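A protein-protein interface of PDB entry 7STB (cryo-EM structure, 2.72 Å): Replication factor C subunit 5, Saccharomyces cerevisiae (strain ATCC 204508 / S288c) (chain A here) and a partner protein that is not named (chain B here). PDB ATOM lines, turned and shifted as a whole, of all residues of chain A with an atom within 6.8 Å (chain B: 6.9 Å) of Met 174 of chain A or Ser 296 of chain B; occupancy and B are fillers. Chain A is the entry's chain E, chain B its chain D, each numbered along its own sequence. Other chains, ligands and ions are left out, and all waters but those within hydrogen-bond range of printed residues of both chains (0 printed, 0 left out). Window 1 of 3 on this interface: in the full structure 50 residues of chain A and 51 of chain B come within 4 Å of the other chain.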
ATOM      1  N   LEU A  40       2.062  12.264 -13.658  1.00  0.00           N
ATOM      2  CA  LEU A  40       1.538  12.253 -15.020  1.00  0.00           C
ATOM      3  C   LEU A  40       0.648  11.026 -15.158  1.00  0.00           C
ATOM      4  O   LEU A  40       1.147   9.899 -15.233  1.00  0.00           O
ATOM      5  CB  LEU A  40       2.667  12.234 -16.052  1.00  0.00           C
ATOM      6  CG  LEU A  40       2.255  12.097 -17.520  1.00  0.00           C
ATOM      7  CD1 LEU A  40       1.411  13.280 -17.963  1.00  0.00           C
ATOM      8  CD2 LEU A  40       3.482  11.958 -18.406  1.00  0.00           C
ATOM      9  N   LEU A  41      -0.663  11.244 -15.171  1.00  0.00           N
ATOM     10  CA  LEU A  41      -1.640  10.171 -15.299  1.00  0.00           C
ATOM     11  C   LEU A  41      -1.982   9.984 -16.771  1.00  0.00           C
ATOM     12  O   LEU A  41      -2.550  10.884 -17.399  1.00  0.00           O
ATOM     13  CB  LEU A  41      -2.901  10.491 -14.497  1.00  0.00           C
ATOM     14  CG  LEU A  41      -2.851  10.218 -12.994  1.00  0.00           C
ATOM     15  CD1 LEU A  41      -2.084  11.314 -12.273  1.00  0.00           C
ATOM     16  CD2 LEU A  41      -4.256  10.086 -12.430  1.00  0.00           C
ATOM     17  N   TYR A  42      -1.646   8.818 -17.314  1.00  0.00           N
ATOM     18  CA  TYR A  42      -1.953   8.484 -18.698  1.00  0.00           C
ATOM     19  C   TYR A  42      -2.950   7.336 -18.732  1.00  0.00           C
ATOM     20  O   TYR A  42      -2.796   6.347 -18.006  1.00  0.00           O
ATOM     21  CB  TYR A  42      -0.685   8.125 -19.479  1.00  0.00           C
ATOM     22  CG  TYR A  42       0.052   6.904 -18.984  1.00  0.00           C
ATOM     23  CD1 TYR A  42       0.917   6.982 -17.903  1.00  0.00           C
ATOM     24  CD2 TYR A  42      -0.100   5.676 -19.612  1.00  0.00           C
ATOM     25  CE1 TYR A  42       1.599   5.871 -17.453  1.00  0.00           C
ATOM     26  CE2 TYR A  42       0.578   4.559 -19.169  1.00  0.00           C
ATOM     27  CZ  TYR A  42       1.427   4.662 -18.090  1.00  0.00           C
ATOM     28  OH  TYR A  42       2.107   3.553 -17.643  1.00  0.00           O
ATOM     29  N   ASN A 144      -0.875  15.740 -23.486  1.00  0.00           N
ATOM     30  CA  ASN A 144      -0.306  15.284 -24.748  1.00  0.00           C
ATOM     31  C   ASN A 144      -0.547  16.260 -25.891  1.00  0.00           C
ATOM     32  O   ASN A 144       0.095  16.126 -26.939  1.00  0.00           O
ATOM     33  CB  ASN A 144      -0.878  13.914 -25.115  1.00  0.00           C
ATOM     34  CG  ASN A 144      -2.387  13.925 -25.239  1.00  0.00           C
ATOM     35  OD1 ASN A 144      -3.058  14.822 -24.731  1.00  0.00           O
ATOM     36  ND2 ASN A 144      -2.931  12.923 -25.920  1.00  0.00           N
ATOM     37  N   CYS A 171      -3.233  12.796 -19.480  1.00  0.00           N
ATOM     38  CA  CYS A 171      -3.153  12.554 -20.913  1.00  0.00           C
ATOM     39  C   CYS A 171      -3.771  11.205 -21.257  1.00  0.00           C
ATOM     40  O   CYS A 171      -3.906  10.316 -20.411  1.00  0.00           O
ATOM     41  CB  CYS A 171      -1.702  12.611 -21.408  1.00  0.00           C
ATOM     42  SG  CYS A 171      -0.661  11.258 -20.819  1.00  0.00           S
ATOM     43  N   ASP A 172      -4.146  11.070 -22.527  1.00  0.00           N
ATOM     44  CA  ASP A 172      -4.627   9.810 -23.071  1.00  0.00           C
ATOM     45  C   ASP A 172      -3.559   9.054 -23.849  1.00  0.00           C
ATOM     46  O   ASP A 172      -3.739   7.862 -24.121  1.00  0.00           O
ATOM     47  CB  ASP A 172      -5.842  10.054 -23.977  1.00  0.00           C
ATOM     48  CG  ASP A 172      -5.509  10.910 -25.186  1.00  0.00           C
ATOM     49  OD1 ASP A 172      -4.347  11.351 -25.308  1.00  0.00           O
ATOM     50  OD2 ASP A 172      -6.413  11.143 -26.016  1.00  0.00           O
ATOM     51  N   SER A 173      -2.458   9.712 -24.207  1.00  0.00           N
ATOM     52  CA  SER A 173      -1.380   9.077 -24.953  1.00  0.00           C
ATOM     53  C   SER A 173      -0.070   9.757 -24.589  1.00  0.00           C
ATOM     54  O   SER A 173       0.031  10.984 -24.656  1.00  0.00           O
ATOM     55  CB  SER A 173      -1.628   9.167 -26.461  1.00  0.00           C
ATOM     56  OG  SER A 173      -1.975  10.488 -26.843  1.00  0.00           O
ATOM     57  N   MET A 174       0.925   8.959 -24.206  1.00  0.00           N
ATOM     58  CA  MET A 174       2.235   9.477 -23.840  1.00  0.00           C
ATOM     59  C   MET A 174       3.165   9.637 -25.036  1.00  0.00           C
ATOM     60  O   MET A 174       4.286  10.124 -24.867  1.00  0.00           O
ATOM     61  CB  MET A 174       2.892   8.559 -22.804  1.00  0.00           C
ATOM     62  CG  MET A 174       2.453   8.828 -21.373  1.00  0.00           C
ATOM     63  SD  MET A 174       3.587   8.141 -20.153  1.00  0.00           S
ATOM     64  CE  MET A 174       3.718   6.448 -20.720  1.00  0.00           C
ATOM     65  N   SER A 175       2.733   9.239 -26.231  1.00  0.00           N
ATOM     66  CA  SER A 175       3.594   9.359 -27.405  1.00  0.00           C
ATOM     67  C   SER A 175       3.992  10.802 -27.690  1.00  0.00           C
ATOM     68  O   SER A 175       5.180  11.047 -27.963  1.00  0.00           O
ATOM     69  CB  SER A 175       2.901   8.720 -28.614  1.00  0.00           C
ATOM     70  OG  SER A 175       3.519   9.115 -29.825  1.00  0.00           O
ATOM     71  N   PRO A 176       3.092  11.785 -27.649  1.00  0.00           N
ATOM     72  CA  PRO A 176       3.486  13.172 -27.926  1.00  0.00           C
ATOM     73  C   PRO A 176       4.182  13.879 -26.772  1.00  0.00           C
ATOM     74  O   PRO A 176       4.347  15.100 -26.837  1.00  0.00           O
ATOM     75  CB  PRO A 176       2.142  13.857 -28.244  1.00  0.00           C
ATOM     76  CG  PRO A 176       1.120  12.758 -28.327  1.00  0.00           C
ATOM     77  CD  PRO A 176       1.638  11.671 -27.462  1.00  0.00           C
ATOM     78  N   ILE A 177       4.590  13.164 -25.726  1.00  0.00           N
ATOM     79  CA  ILE A 177       5.279  13.753 -24.583  1.00  0.00           C
ATOM     80  C   ILE A 177       6.777  13.567 -24.778  1.00  0.00           C
ATOM     81  O   ILE A 177       7.245  12.449 -25.025  1.00  0.00           O
ATOM     82  CB  ILE A 177       4.815  13.121 -23.260  1.00  0.00           C
ATOM     83  CG1 ILE A 177       3.293  13.236 -23.104  1.00  0.00           C
ATOM     84  CG2 ILE A 177       5.525  13.775 -22.082  1.00  0.00           C
ATOM     85  CD1 ILE A 177       2.799  14.642 -22.833  1.00  0.00           C
ATOM     86  N   ILE A 178       7.532  14.663 -24.664  1.00  0.00           N
ATOM     87  CA  ILE A 178       8.974  14.595 -24.861  1.00  0.00           C
ATOM     88  C   ILE A 178       9.615  13.808 -23.723  1.00  0.00           C
ATOM     89  O   ILE A 178       9.079  13.721 -22.611  1.00  0.00           O
ATOM     90  CB  ILE A 178       9.578  16.006 -24.974  1.00  0.00           C
ATOM     91  CG1 ILE A 178       9.353  16.802 -23.684  1.00  0.00           C
ATOM     92  CG2 ILE A 178       8.976  16.742 -26.159  1.00  0.00           C
ATOM     93  CD1 ILE A 178      10.079  18.132 -23.653  1.00  0.00           C
ATOM     94  N   LYS A 182       8.654  13.143 -19.367  1.00  0.00           N
ATOM     95  CA  LYS A 182       8.410  11.822 -18.802  1.00  0.00           C
ATOM     96  C   LYS A 182       9.451  11.474 -17.750  1.00  0.00           C
ATOM     97  O   LYS A 182       9.134  10.810 -16.756  1.00  0.00           O
ATOM     98  CB  LYS A 182       8.397  10.770 -19.912  1.00  0.00           C
ATOM     99  CG  LYS A 182       7.129  10.781 -20.750  1.00  0.00           C
ATOM    100  CD  LYS A 182       7.379  10.273 -22.161  1.00  0.00           C
ATOM    101  CE  LYS A 182       7.692   8.786 -22.178  1.00  0.00           C
ATOM    102  NZ  LYS A 182       6.556   7.964 -21.679  1.00  0.00           N
ATOM    103  N   LEU A 187       5.034   8.442 -13.583  1.00  0.00           N
ATOM    104  CA  LEU A 187       4.008   7.953 -14.496  1.00  0.00           C
ATOM    105  C   LEU A 187       2.993   7.097 -13.749  1.00  0.00           C
ATOM    106  O   LEU A 187       3.363   6.240 -12.941  1.00  0.00           O
ATOM    107  CB  LEU A 187       4.648   7.147 -15.626  1.00  0.00           C
ATOM    108  CG  LEU A 187       5.819   7.818 -16.347  1.00  0.00           C
ATOM    109  CD1 LEU A 187       6.266   6.977 -17.532  1.00  0.00           C
ATOM    110  CD2 LEU A 187       5.450   9.222 -16.795  1.00  0.00           C
ATOM    111  N   ILE A 188       1.710   7.331 -14.023  1.00  0.00           N
ATOM    112  CA  ILE A 188       0.618   6.577 -13.419  1.00  0.00           C
ATOM    113  C   ILE A 188      -0.305   6.109 -14.536  1.00  0.00           C
ATOM    114  O   ILE A 188      -0.909   6.933 -15.233  1.00  0.00           O
ATOM    115  CB  ILE A 188      -0.163   7.412 -12.389  1.00  0.00           C
ATOM    116  CG1 ILE A 188       0.790   7.994 -11.340  1.00  0.00           C
ATOM    117  CG2 ILE A 188      -1.240   6.567 -11.722  1.00  0.00           C
ATOM    118  CD1 ILE A 188       0.143   8.989 -10.405  1.00  0.00           C
ATOM    119  N   ARG A 189      -0.430   4.794 -14.691  1.00  0.00           N
ATOM    120  CA  ARG A 189      -1.317   4.210 -15.687  1.00  0.00           C
ATOM    121  C   ARG A 189      -2.727   4.111 -15.118  1.00  0.00           C
ATOM    122  O   ARG A 189      -2.912   3.673 -13.979  1.00  0.00           O
ATOM    123  CB  ARG A 189      -0.818   2.828 -16.105  1.00  0.00           C
ATOM    124  CG  ARG A 189      -1.555   2.230 -17.289  1.00  0.00           C
ATOM    125  CD  ARG A 189      -0.989   0.871 -17.655  1.00  0.00           C
ATOM    126  NE  ARG A 189      -1.045  -0.064 -16.536  1.00  0.00           N
ATOM    127  CZ  ARG A 189      -2.002  -0.963 -16.347  1.00  0.00           C
ATOM    128  NH1 ARG A 189      -3.017  -1.087 -17.188  1.00  0.00           N
ATOM    129  NH2 ARG A 189      -1.938  -1.764 -15.287  1.00  0.00           N
ATOM    130  N   ALA B 260       6.352   0.914 -12.796  1.00  0.00           N
ATOM    131  CA  ALA B 260       7.079   1.497 -13.918  1.00  0.00           C
ATOM    132  C   ALA B 260       6.210   1.595 -15.165  1.00  0.00           C
ATOM    133  O   ALA B 260       6.453   2.455 -16.019  1.00  0.00           O
ATOM    134  CB  ALA B 260       8.331   0.673 -14.213  1.00  0.00           C
ATOM    135  N   GLY B 261       5.203   0.738 -15.287  1.00  0.00           N
ATOM    136  CA  GLY B 261       4.376   0.687 -16.472  1.00  0.00           C
ATOM    137  C   GLY B 261       4.768  -0.371 -17.479  1.00  0.00           C
ATOM    138  O   GLY B 261       4.256  -0.347 -18.603  1.00  0.00           O
ATOM    139  N   VAL B 263       4.655  -3.689 -19.459  1.00  0.00           N
ATOM    140  CA  VAL B 263       3.580  -4.652 -19.721  1.00  0.00           C
ATOM    141  C   VAL B 263       3.968  -6.004 -19.134  1.00  0.00           C
ATOM    142  O   VAL B 263       5.130  -6.432 -19.286  1.00  0.00           O
ATOM    143  CB  VAL B 263       3.309  -4.764 -21.231  1.00  0.00           C
ATOM    144  CG1 VAL B 263       2.212  -5.779 -21.504  1.00  0.00           C
ATOM    145  CG2 VAL B 263       2.938  -3.406 -21.805  1.00  0.00           C
ATOM    146  N   PHE B 290      -6.464  -4.966 -25.541  1.00  0.00           N
ATOM    147  CA  PHE B 290      -5.223  -4.593 -24.868  1.00  0.00           C
ATOM    148  C   PHE B 290      -5.096  -3.080 -24.741  1.00  0.00           C
ATOM    149  O   PHE B 290      -4.737  -2.564 -23.676  1.00  0.00           O
ATOM    150  CB  PHE B 290      -4.033  -5.176 -25.632  1.00  0.00           C
ATOM    151  CG  PHE B 290      -2.705  -4.594 -25.234  1.00  0.00           C
ATOM    152  CD1 PHE B 290      -1.951  -5.178 -24.230  1.00  0.00           C
ATOM    153  CD2 PHE B 290      -2.201  -3.473 -25.876  1.00  0.00           C
ATOM    154  CE1 PHE B 290      -0.728  -4.651 -23.867  1.00  0.00           C
ATOM    155  CE2 PHE B 290      -0.979  -2.940 -25.513  1.00  0.00           C
ATOM    156  CZ  PHE B 290      -0.242  -3.531 -24.509  1.00  0.00           C
ATOM    157  N   MET B 291      -5.387  -2.350 -25.819  1.00  0.00           N
ATOM    158  CA  MET B 291      -5.242  -0.901 -25.804  1.00  0.00           C
ATOM    159  C   MET B 291      -6.325  -0.225 -24.980  1.00  0.00           C
ATOM    160  O   MET B 291      -6.170   0.948 -24.621  1.00  0.00           O
ATOM    161  CB  MET B 291      -5.255  -0.359 -27.233  1.00  0.00           C
ATOM    162  CG  MET B 291      -4.061  -0.799 -28.068  1.00  0.00           C
ATOM    163  SD  MET B 291      -2.483  -0.250 -27.392  1.00  0.00           S
ATOM    164  CE  MET B 291      -2.592   1.515 -27.673  1.00  0.00           C
ATOM    165  N   GLY B 294      -4.779   0.926 -21.284  1.00  0.00           N
ATOM    166  CA  GLY B 294      -3.959   2.084 -20.996  1.00  0.00           C
ATOM    167  C   GLY B 294      -2.466   1.889 -21.141  1.00  0.00           C
ATOM    168  O   GLY B 294      -1.708   2.812 -20.821  1.00  0.00           O
ATOM    169  N   TRP B 295      -2.016   0.731 -21.617  1.00  0.00           N
ATOM    170  CA  TRP B 295      -0.587   0.498 -21.773  1.00  0.00           C
ATOM    171  C   TRP B 295       0.003   1.439 -22.816  1.00  0.00           C
ATOM    172  O   TRP B 295      -0.671   1.868 -23.757  1.00  0.00           O
ATOM    173  CB  TRP B 295      -0.320  -0.951 -22.177  1.00  0.00           C
ATOM    174  CG  TRP B 295      -0.858  -1.957 -21.211  1.00  0.00           C
ATOM    175  CD1 TRP B 295      -1.923  -2.787 -21.400  1.00  0.00           C
ATOM    176  CD2 TRP B 295      -0.352  -2.246 -19.902  1.00  0.00           C
ATOM    177  NE1 TRP B 295      -2.112  -3.573 -20.289  1.00  0.00           N
ATOM    178  CE2 TRP B 295      -1.161  -3.260 -19.356  1.00  0.00           C
ATOM    179  CE3 TRP B 295       0.707  -1.744 -19.140  1.00  0.00           C
ATOM    180  CZ2 TRP B 295      -0.944  -3.782 -18.083  1.00  0.00           C
ATOM    181  CZ3 TRP B 295       0.919  -2.263 -17.878  1.00  0.00           C
ATOM    182  CH2 TRP B 295       0.098  -3.270 -17.361  1.00  0.00           C
ATOM    183  N   SER B 296       1.281   1.763 -22.638  1.00  0.00           N
ATOM    184  CA  SER B 296       1.999   2.624 -23.566  1.00  0.00           C
ATOM    185  C   SER B 296       2.581   1.797 -24.705  1.00  0.00           C
ATOM    186  O   SER B 296       3.078   0.687 -24.493  1.00  0.00           O
ATOM    187  CB  SER B 296       3.116   3.380 -22.846  1.00  0.00           C
ATOM    188  OG  SER B 296       3.811   4.233 -23.739  1.00  0.00           O
ATOM    189  N   ALA B 297       2.512   2.347 -25.919  1.00  0.00           N
ATOM    190  CA  ALA B 297       3.013   1.624 -27.083  1.00  0.00           C
ATOM    191  C   ALA B 297       4.529   1.495 -27.060  1.00  0.00           C
ATOM    192  O   ALA B 297       5.070   0.494 -27.541  1.00  0.00           O
ATOM    193  CB  ALA B 297       2.570   2.318 -28.368  1.00  0.00           C
ATOM    194  N   ALA B 298       5.232   2.493 -26.522  1.00  0.00           N
ATOM    195  CA  ALA B 298       6.689   2.434 -26.497  1.00  0.00           C
ATOM    196  C   ALA B 298       7.181   1.254 -25.667  1.00  0.00           C
ATOM    197  O   ALA B 298       8.102   0.539 -26.077  1.00  0.00           O
ATOM    198  CB  ALA B 298       7.256   3.745 -25.954  1.00  0.00           C
ATOM    199  N   SER B 299       6.574   1.033 -24.499  1.00  0.00           N
ATOM    200  CA  SER B 299       7.019  -0.053 -23.631  1.00  0.00           C
ATOM    201  C   SER B 299       6.792  -1.409 -24.286  1.00  0.00           C
ATOM    202  O   SER B 299       7.674  -2.278 -24.267  1.00  0.00           O
ATOM    203  CB  SER B 299       6.291   0.026 -22.289  1.00  0.00           C
ATOM    204  OG  SER B 299       6.534   1.267 -21.650  1.00  0.00           O
ATOM    205  N   VAL B 300       5.611  -1.611 -24.873  1.00  0.00           N
ATOM    206  CA  VAL B 300       5.316  -2.895 -25.502  1.00  0.00           C
ATOM    207  C   VAL B 300       6.193  -3.100 -26.729  1.00  0.00           C
ATOM    208  O   VAL B 300       6.625  -4.221 -27.015  1.00  0.00           O
ATOM    209  CB  VAL B 300       3.817  -2.998 -25.845  1.00  0.00           C
ATOM    210  CG1 VAL B 300       3.424  -1.960 -26.879  1.00  0.00           C
ATOM    211  CG2 VAL B 300       3.480  -4.399 -26.335  1.00  0.00           C
ATOM    212  N   VAL B 301       6.473  -2.028 -27.473  1.00  0.00           N
ATOM    213  CA  VAL B 301       7.355  -2.145 -28.632  1.00  0.00           C
ATOM    214  C   VAL B 301       8.759  -2.538 -28.192  1.00  0.00           C
ATOM    215  O   VAL B 301       9.403  -3.395 -28.809  1.00  0.00           O
ATOM    216  CB  VAL B 301       7.358  -0.832 -29.436  1.00  0.00           C
ATOM    217  CG1 VAL B 301       8.554  -0.780 -30.374  1.00  0.00           C
ATOM    218  CG2 VAL B 301       6.061  -0.691 -30.216  1.00  0.00           C
ATOM    219  N   LEU B 333       6.113   6.382 -33.727  1.00  0.00           N
ATOM    220  CA  LEU B 333       5.613   6.701 -32.394  1.00  0.00           C
ATOM    221  C   LEU B 333       6.265   7.965 -31.849  1.00  0.00           C
ATOM    222  O   LEU B 333       5.593   8.801 -31.233  1.00  0.00           O
ATOM    223  CB  LEU B 333       5.853   5.526 -31.449  1.00  0.00           C
ATOM    224  CG  LEU B 333       4.959   4.304 -31.664  1.00  0.00           C
ATOM    225  CD1 LEU B 333       5.504   3.111 -30.897  1.00  0.00           C
ATOM    226  CD2 LEU B 333       3.526   4.598 -31.251  1.00  0.00           C
ATOM    227  N   GLU B 339      -1.286   5.509 -30.989  1.00  0.00           N
ATOM    228  CA  GLU B 339      -0.649   4.278 -30.535  1.00  0.00           C
ATOM    229  C   GLU B 339      -1.418   3.049 -31.005  1.00  0.00           C
ATOM    230  O   GLU B 339      -0.818   2.033 -31.371  1.00  0.00           O
ATOM    231  CB  GLU B 339      -0.532   4.288 -29.012  1.00  0.00           C
ATOM    232  CG  GLU B 339       0.596   5.163 -28.489  1.00  0.00           C
ATOM    233  CD  GLU B 339       0.411   5.550 -27.035  1.00  0.00           C
ATOM    234  OE1 GLU B 339       0.597   4.679 -26.160  1.00  0.00           O
ATOM    235  OE2 GLU B 339       0.087   6.726 -26.767  1.00  0.00           O
ATOM    236  N   LEU B 343       0.349   0.190 -33.280  1.00  0.00           N
ATOM    237  CA  LEU B 343       0.520  -1.138 -32.702  1.00  0.00           C
ATOM    238  C   LEU B 343      -0.169  -2.197 -33.552  1.00  0.00           C
ATOM    239  O   LEU B 343       0.391  -3.277 -33.788  1.00  0.00           O
ATOM    240  CB  LEU B 343      -0.021  -1.162 -31.272  1.00  0.00           C
ATOM    241  CG  LEU B 343       0.263  -2.436 -30.472  1.00  0.00           C
ATOM    242  CD1 LEU B 343       1.758  -2.629 -30.268  1.00  0.00           C
ATOM    243  CD2 LEU B 343      -0.461  -2.401 -29.136  1.00  0.00           C
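OG of Ser 175 of chain A is in hydrogen-bond range of O of Leu 333 of chain B (2.5 Å).
The backbone NH of Met 174 of chain A is in hydrogen-bond range of the side-chain carboxylate of Glu 339 of chain B.
OE1 of Glu 339 of chain B lies within hydrogen-bond range of N of Ala 297 of chain B (3.0 Å).
N of Tyr 42 of chain A sits at hydrogen-bond distance from O of Ile 188 of chain A (2.9 Å).
The side-chain amide nitrogen (ND2) of Asn 144 of chain A sits at hydrogen-bond distance from the side-chain hydroxyl (OG) of Ser 173 of chain A, at 2.8 Å.
OD1 of Asp 172 of chain A lies within hydrogen-bond range of OG of Ser 173 of chain A, at 3.0 Å.
The side-chain sulfur (SD) of Met 174 of chain A is in hydrogen-bond range of the side-chain amino group (NZ) of Lys 182 of chain A, 3.3 Å away.
Tyr 42 of chain A touches Gly 261 of chain B (OH to CA, 3.8 Å).
O of Gly 294 of chain B touches CE2 of Tyr 42 of chain A (3.3 Å).
Ser 173 of chain A touches Glu 339 of chain B (CB to OE2, 3.0 Å).
Met 174 of chain A touches Ser 296 of chain B.
Glu 339 of chain B touches Ser 175 of chain A.
CG of Arg 189 of chain A touches O of Gly 294 of chain B (3.6 Å).
NE of Arg 189 of chain A touches CZ3 of Trp 295 of chain B, 3.2 Å away.
Printed residues of chain B within 4 Å of Met 174 of chain A: Ser 296 and Glu 339.
Ser 296 of chain B touches just one residue of chain A: Met 174.
Of the printed residues of chain B, Arg 189 of chain A touches Gly 294 (3.6 Å) and Trp 295 (3.2 Å).
Printed residues of chain B within 4 Å of Tyr 42 of chain A: Gly 261 and Gly 294.
Lys 182 of chain A touches none of the printed residues of chain B.
The nearest residue of chain B that does not touch Met 174 of chain A is Ser 299 of chain B (6.0 Å).
The nearest residue of chain A that does not touch Ser 296 of chain B is Tyr 42 of chain A (4.5 Å).
The nearest printed residue of chain B that does not touch Ser 175 of chain A is Ser 296 of chain B (5.7 Å).
Hydrophobic or aromatic side chains of chain B that line the printed part of chain A: Trp 295.
Of the 16 printed residues of chain A, 5 touch a printed residue of chain B.
Printed residues of chain A that touch a printed residue of chain B: Tyr 42, Ser 173, Met 174, Ser 175 and Arg 189.
Hydrophobic or aromatic side chains of chain A within 4 Å of the printed part of chain B: Tyr 42 and Met 174.
Among the printed residues, no Asp or Glu carboxylate lies within 4 Å of a Lys or Arg side-chain nitrogen of the other chain.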
